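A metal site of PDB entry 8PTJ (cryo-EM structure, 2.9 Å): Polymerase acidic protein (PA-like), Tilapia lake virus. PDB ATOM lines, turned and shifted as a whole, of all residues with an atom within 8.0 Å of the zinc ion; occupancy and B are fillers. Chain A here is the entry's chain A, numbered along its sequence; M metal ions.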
ATOM      1  N   PHE A 159      -7.606 -17.203  14.105  1.00  0.00           N
ATOM      2  CA  PHE A 159      -8.981 -17.267  14.568  1.00  0.00           C
ATOM      3  C   PHE A 159      -9.054 -18.050  15.879  1.00  0.00           C
ATOM      4  O   PHE A 159      -8.148 -18.804  16.237  1.00  0.00           O
ATOM      5  CB  PHE A 159      -9.872 -17.937  13.528  1.00  0.00           C
ATOM      6  CG  PHE A 159     -10.510 -16.972  12.567  1.00  0.00           C
ATOM      7  CD1 PHE A 159     -11.342 -15.959  13.021  1.00  0.00           C
ATOM      8  CD2 PHE A 159     -10.299 -17.101  11.202  1.00  0.00           C
ATOM      9  CE1 PHE A 159     -11.930 -15.082  12.135  1.00  0.00           C
ATOM     10  CE2 PHE A 159     -10.887 -16.225  10.316  1.00  0.00           C
ATOM     11  CZ  PHE A 159     -11.700 -15.216  10.778  1.00  0.00           C
ATOM     12  N   GLU A 160     -10.159 -17.849  16.601  1.00  0.00           N
ATOM     13  CA  GLU A 160     -10.342 -18.568  17.863  1.00  0.00           C
ATOM     14  C   GLU A 160     -10.714 -20.022  17.626  1.00  0.00           C
ATOM     15  O   GLU A 160     -10.281 -20.904  18.372  1.00  0.00           O
ATOM     16  CB  GLU A 160     -11.420 -17.871  18.698  1.00  0.00           C
ATOM     17  CG  GLU A 160     -11.067 -16.451  19.104  1.00  0.00           C
ATOM     18  CD  GLU A 160      -9.762 -16.363  19.869  1.00  0.00           C
ATOM     19  OE1 GLU A 160      -9.487 -17.286  20.662  1.00  0.00           O
ATOM     20  OE2 GLU A 160      -9.023 -15.377  19.677  1.00  0.00           O
ATOM     21  N   CYS A 161     -11.516 -20.290  16.598  1.00  0.00           N
ATOM     22  CA  CYS A 161     -11.930 -21.640  16.244  1.00  0.00           C
ATOM     23  C   CYS A 161     -11.535 -21.932  14.799  1.00  0.00           C
ATOM     24  O   CYS A 161     -11.086 -21.052  14.059  1.00  0.00           O
ATOM     25  CB  CYS A 161     -13.432 -21.828  16.434  1.00  0.00           C
ATOM     26  SG  CYS A 161     -14.459 -20.811  15.347  1.00  0.00           S
ATOM     27  N   SER A 162     -11.727 -23.183  14.402  1.00  0.00           N
ATOM     28  CA  SER A 162     -11.340 -23.630  13.065  1.00  0.00           C
ATOM     29  C   SER A 162     -12.402 -23.344  12.016  1.00  0.00           C
ATOM     30  O   SER A 162     -12.164 -23.591  10.830  1.00  0.00           O
ATOM     31  CB  SER A 162     -11.037 -25.132  13.089  1.00  0.00           C
ATOM     32  OG  SER A 162      -9.825 -25.388  13.768  1.00  0.00           O
ATOM     33  N   LYS A 163     -13.563 -22.825  12.410  1.00  0.00           N
ATOM     34  CA  LYS A 163     -14.611 -22.431  11.467  1.00  0.00           C
ATOM     35  C   LYS A 163     -15.007 -23.665  10.651  1.00  0.00           C
ATOM     36  O   LYS A 163     -15.082 -24.770  11.207  1.00  0.00           O
ATOM     37  CB  LYS A 163     -14.139 -21.242  10.664  1.00  0.00           C
ATOM     38  CG  LYS A 163     -13.809 -20.022  11.502  1.00  0.00           C
ATOM     39  CD  LYS A 163     -14.746 -18.862  11.241  1.00  0.00           C
ATOM     40  CE  LYS A 163     -14.190 -17.939  10.167  1.00  0.00           C
ATOM     41  NZ  LYS A 163     -15.137 -16.856   9.806  1.00  0.00           N
ATOM     42  N   PHE A 164     -15.254 -23.517   9.347  1.00  0.00           N
ATOM     43  CA  PHE A 164     -15.737 -24.646   8.558  1.00  0.00           C
ATOM     44  C   PHE A 164     -14.754 -25.806   8.535  1.00  0.00           C
ATOM     45  O   PHE A 164     -15.161 -26.943   8.301  1.00  0.00           O
ATOM     46  CB  PHE A 164     -16.035 -24.197   7.124  1.00  0.00           C
ATOM     47  CG  PHE A 164     -16.980 -25.109   6.403  1.00  0.00           C
ATOM     48  CD1 PHE A 164     -18.350 -24.961   6.544  1.00  0.00           C
ATOM     49  CD2 PHE A 164     -16.502 -26.107   5.572  1.00  0.00           C
ATOM     50  CE1 PHE A 164     -19.224 -25.793   5.879  1.00  0.00           C
ATOM     51  CE2 PHE A 164     -17.364 -26.942   4.902  1.00  0.00           C
ATOM     52  CZ  PHE A 164     -18.727 -26.795   5.056  1.00  0.00           C
ATOM     53  N   ALA A 166     -13.532 -27.205  10.934  1.00  0.00           N
ATOM     54  CA  ALA A 166     -13.920 -28.117  12.002  1.00  0.00           C
ATOM     55  C   ALA A 166     -15.062 -29.040  11.610  1.00  0.00           C
ATOM     56  O   ALA A 166     -15.364 -29.964  12.368  1.00  0.00           O
ATOM     57  CB  ALA A 166     -14.317 -27.313  13.247  1.00  0.00           C
ATOM     58  N   SER A 278     -20.496 -28.599  13.772  1.00  0.00           N
ATOM     59  CA  SER A 278     -19.340 -29.173  14.427  1.00  0.00           C
ATOM     60  C   SER A 278     -19.585 -29.160  15.926  1.00  0.00           C
ATOM     61  O   SER A 278     -20.599 -28.658  16.408  1.00  0.00           O
ATOM     62  CB  SER A 278     -18.054 -28.412  14.058  1.00  0.00           C
ATOM     63  OG  SER A 278     -18.289 -27.018  14.054  1.00  0.00           O
ATOM     64  N   LYS A 279     -18.630 -29.710  16.688  1.00  0.00           N
ATOM     65  CA  LYS A 279     -18.777 -29.765  18.126  1.00  0.00           C
ATOM     66  C   LYS A 279     -18.886 -28.358  18.703  1.00  0.00           C
ATOM     67  O   LYS A 279     -18.270 -27.418  18.184  1.00  0.00           O
ATOM     68  CB  LYS A 279     -17.600 -30.490  18.759  1.00  0.00           C
ATOM     69  CG  LYS A 279     -17.406 -31.922  18.261  1.00  0.00           C
ATOM     70  CD  LYS A 279     -17.383 -32.925  19.405  1.00  0.00           C
ATOM     71  CE  LYS A 279     -16.423 -34.069  19.113  1.00  0.00           C
ATOM     72  NZ  LYS A 279     -16.883 -34.929  17.989  1.00  0.00           N
ATOM     73  N   PRO A 280     -19.664 -28.169  19.758  1.00  0.00           N
ATOM     74  CA  PRO A 280     -19.816 -26.824  20.328  1.00  0.00           C
ATOM     75  C   PRO A 280     -18.606 -26.430  21.161  1.00  0.00           C
ATOM     76  O   PRO A 280     -17.739 -27.239  21.481  1.00  0.00           O
ATOM     77  CB  PRO A 280     -21.077 -26.946  21.195  1.00  0.00           C
ATOM     78  CG  PRO A 280     -21.301 -28.412  21.412  1.00  0.00           C
ATOM     79  CD  PRO A 280     -20.319 -29.189  20.587  1.00  0.00           C
ATOM     80  N   GLY A 281     -18.567 -25.145  21.519  1.00  0.00           N
ATOM     81  CA  GLY A 281     -17.508 -24.633  22.355  1.00  0.00           C
ATOM     82  C   GLY A 281     -16.753 -23.477  21.734  1.00  0.00           C
ATOM     83  O   GLY A 281     -15.587 -23.232  22.070  1.00  0.00           O
ATOM     84  N   CYS A 282     -17.391 -22.755  20.811  1.00  0.00           N
ATOM     85  CA  CYS A 282     -16.779 -21.608  20.161  1.00  0.00           C
ATOM     86  C   CYS A 282     -17.808 -20.485  20.088  1.00  0.00           C
ATOM     87  O   CYS A 282     -18.924 -20.595  20.618  1.00  0.00           O
ATOM     88  CB  CYS A 282     -16.245 -21.960  18.776  1.00  0.00           C
ATOM     89  SG  CYS A 282     -17.499 -22.099  17.490  1.00  0.00           S
ATOM     90  N   GLU A 283     -17.422 -19.389  19.430  1.00  0.00           N
ATOM     91  CA  GLU A 283     -18.301 -18.242  19.320  1.00  0.00           C
ATOM     92  C   GLU A 283     -19.580 -18.584  18.551  1.00  0.00           C
ATOM     93  O   GLU A 283     -20.664 -18.127  18.907  1.00  0.00           O
ATOM     94  CB  GLU A 283     -17.560 -17.086  18.651  1.00  0.00           C
ATOM     95  CG  GLU A 283     -18.427 -15.890  18.259  1.00  0.00           C
ATOM     96  CD  GLU A 283     -17.721 -14.976  17.272  1.00  0.00           C
ATOM     97  OE1 GLU A 283     -16.489 -15.070  17.148  1.00  0.00           O
ATOM     98  OE2 GLU A 283     -18.416 -14.148  16.634  1.00  0.00           O
ATOM     99  N   HIS A 284     -19.454 -19.382  17.498  1.00  0.00           N
ATOM    100  CA  HIS A 284     -20.588 -19.693  16.626  1.00  0.00           C
ATOM    101  C   HIS A 284     -21.395 -20.875  17.168  1.00  0.00           C
ATOM    102  O   HIS A 284     -21.656 -21.844  16.455  1.00  0.00           O
ATOM    103  CB  HIS A 284     -20.102 -19.964  15.210  1.00  0.00           C
ATOM    104  CG  HIS A 284     -18.936 -19.126  14.797  1.00  0.00           C
ATOM    105  ND1 HIS A 284     -17.626 -19.535  14.977  1.00  0.00           N
ATOM    106  CD2 HIS A 284     -18.873 -17.906  14.219  1.00  0.00           C
ATOM    107  CE1 HIS A 284     -16.818 -18.595  14.527  1.00  0.00           C
ATOM    108  NE2 HIS A 284     -17.547 -17.602  14.066  1.00  0.00           N
ATOM    109  N   ASP A 285     -21.803 -20.789  18.426  1.00  0.00           N
ATOM    110  CA  ASP A 285     -22.585 -21.846  19.054  1.00  0.00           C
ATOM    111  C   ASP A 285     -24.077 -21.579  18.874  1.00  0.00           C
ATOM    112  O   ASP A 285     -24.523 -20.426  18.833  1.00  0.00           O
ATOM    113  CB  ASP A 285     -22.248 -21.949  20.544  1.00  0.00           C
ATOM    114  CG  ASP A 285     -21.218 -23.025  20.836  1.00  0.00           C
ATOM    115  OD1 ASP A 285     -21.336 -24.131  20.271  1.00  0.00           O
ATOM    116  OD2 ASP A 285     -20.288 -22.754  21.620  1.00  0.00           O
ATOM    117  N   ALA A 294     -21.835 -26.098  17.010  1.00  0.00           N
ATOM    118  CA  ALA A 294     -21.203 -24.942  16.398  1.00  0.00           C
ATOM    119  C   ALA A 294     -21.581 -24.900  14.924  1.00  0.00           C
ATOM    120  O   ALA A 294     -21.337 -25.857  14.186  1.00  0.00           O
ATOM    121  CB  ALA A 294     -19.684 -25.000  16.565  1.00  0.00           C
ATOM    122  N   VAL A 295     -22.192 -23.798  14.499  1.00  0.00           N
ATOM    123  CA  VAL A 295     -22.675 -23.641  13.131  1.00  0.00           C
ATOM    124  C   VAL A 295     -21.716 -22.726  12.395  1.00  0.00           C
ATOM    125  O   VAL A 295     -21.548 -21.564  12.776  1.00  0.00           O
ATOM    126  CB  VAL A 295     -24.114 -23.087  13.107  1.00  0.00           C
ATOM    127  CG1 VAL A 295     -24.680 -23.169  11.715  1.00  0.00           C
ATOM    128  CG2 VAL A 295     -24.991 -23.827  14.091  1.00  0.00           C
ATOM    129  N   HIS A 296     -21.101 -23.238  11.332  1.00  0.00           N
ATOM    130  CA  HIS A 296     -20.095 -22.501  10.577  1.00  0.00           C
ATOM    131  C   HIS A 296     -20.514 -22.407   9.124  1.00  0.00           C
ATOM    132  O   HIS A 296     -21.000 -23.386   8.535  1.00  0.00           O
ATOM    133  CB  HIS A 296     -18.730 -23.174  10.700  1.00  0.00           C
ATOM    134  CG  HIS A 296     -18.158 -23.125  12.089  1.00  0.00           C
ATOM    135  ND1 HIS A 296     -17.693 -24.237  12.743  1.00  0.00           N
ATOM    136  CD2 HIS A 296     -17.978 -22.085  12.934  1.00  0.00           C
ATOM    137  CE1 HIS A 296     -17.255 -23.892  13.930  1.00  0.00           C
ATOM    138  NE2 HIS A 296     -17.413 -22.587  14.075  1.00  0.00           N
ATOM    139  N   VAL A 297     -20.313 -21.241   8.528  1.00  0.00           N
ATOM    140  CA  VAL A 297     -20.810 -20.945   7.186  1.00  0.00           C
ATOM    141  C   VAL A 297     -19.630 -20.726   6.243  1.00  0.00           C
ATOM    142  O   VAL A 297     -18.516 -20.422   6.658  1.00  0.00           O
ATOM    143  CB  VAL A 297     -21.744 -19.726   7.174  1.00  0.00           C
ATOM    144  CG1 VAL A 297     -22.829 -19.866   8.225  1.00  0.00           C
ATOM    145  CG2 VAL A 297     -20.959 -18.444   7.382  1.00  0.00           C
HETATM  146 ZN    ZN M   1     -16.718 -21.278  15.481  1.00  0.00          ZN
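The backbone NH (N) of Lys 163 lies close to the side-chain sulfur (SG) of Cys 161 (3.7 Å). N of Val 295 lies within hydrogen-bond range of O of His 284 (2.8 Å). N of Cys 282 sits at hydrogen-bond distance from OD2 of Asp 285. A ring nitrogen (ND1) of His 296 lies within hydrogen-bond range of the backbone carbonyl oxygen (O) of Lys 163 (3.1 Å). A ring nitrogen (ND1) of His 296 lies within hydrogen-bond range of the side-chain hydroxyl (OG) of Ser 278 (3.1 Å).
Within 4 Å of the zinc ion: Cys 161, Cys 282, His 284 and His 296. The nearest printed residue that does not touch the zinc ion is Glu 283 (4.4 Å).
A ring nitrogen (ND1) of His 284 is bound to the zinc ion (2.0 Å). The zinc ion is bound by NE2 of His 296. The zinc ion is bound by the side-chain sulfur (SG) of Cys 282, 2.3 Å away. SG of Cys 161 binds the zinc ion (2.3 Å). The zinc ion has four donor atoms within binding distance.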
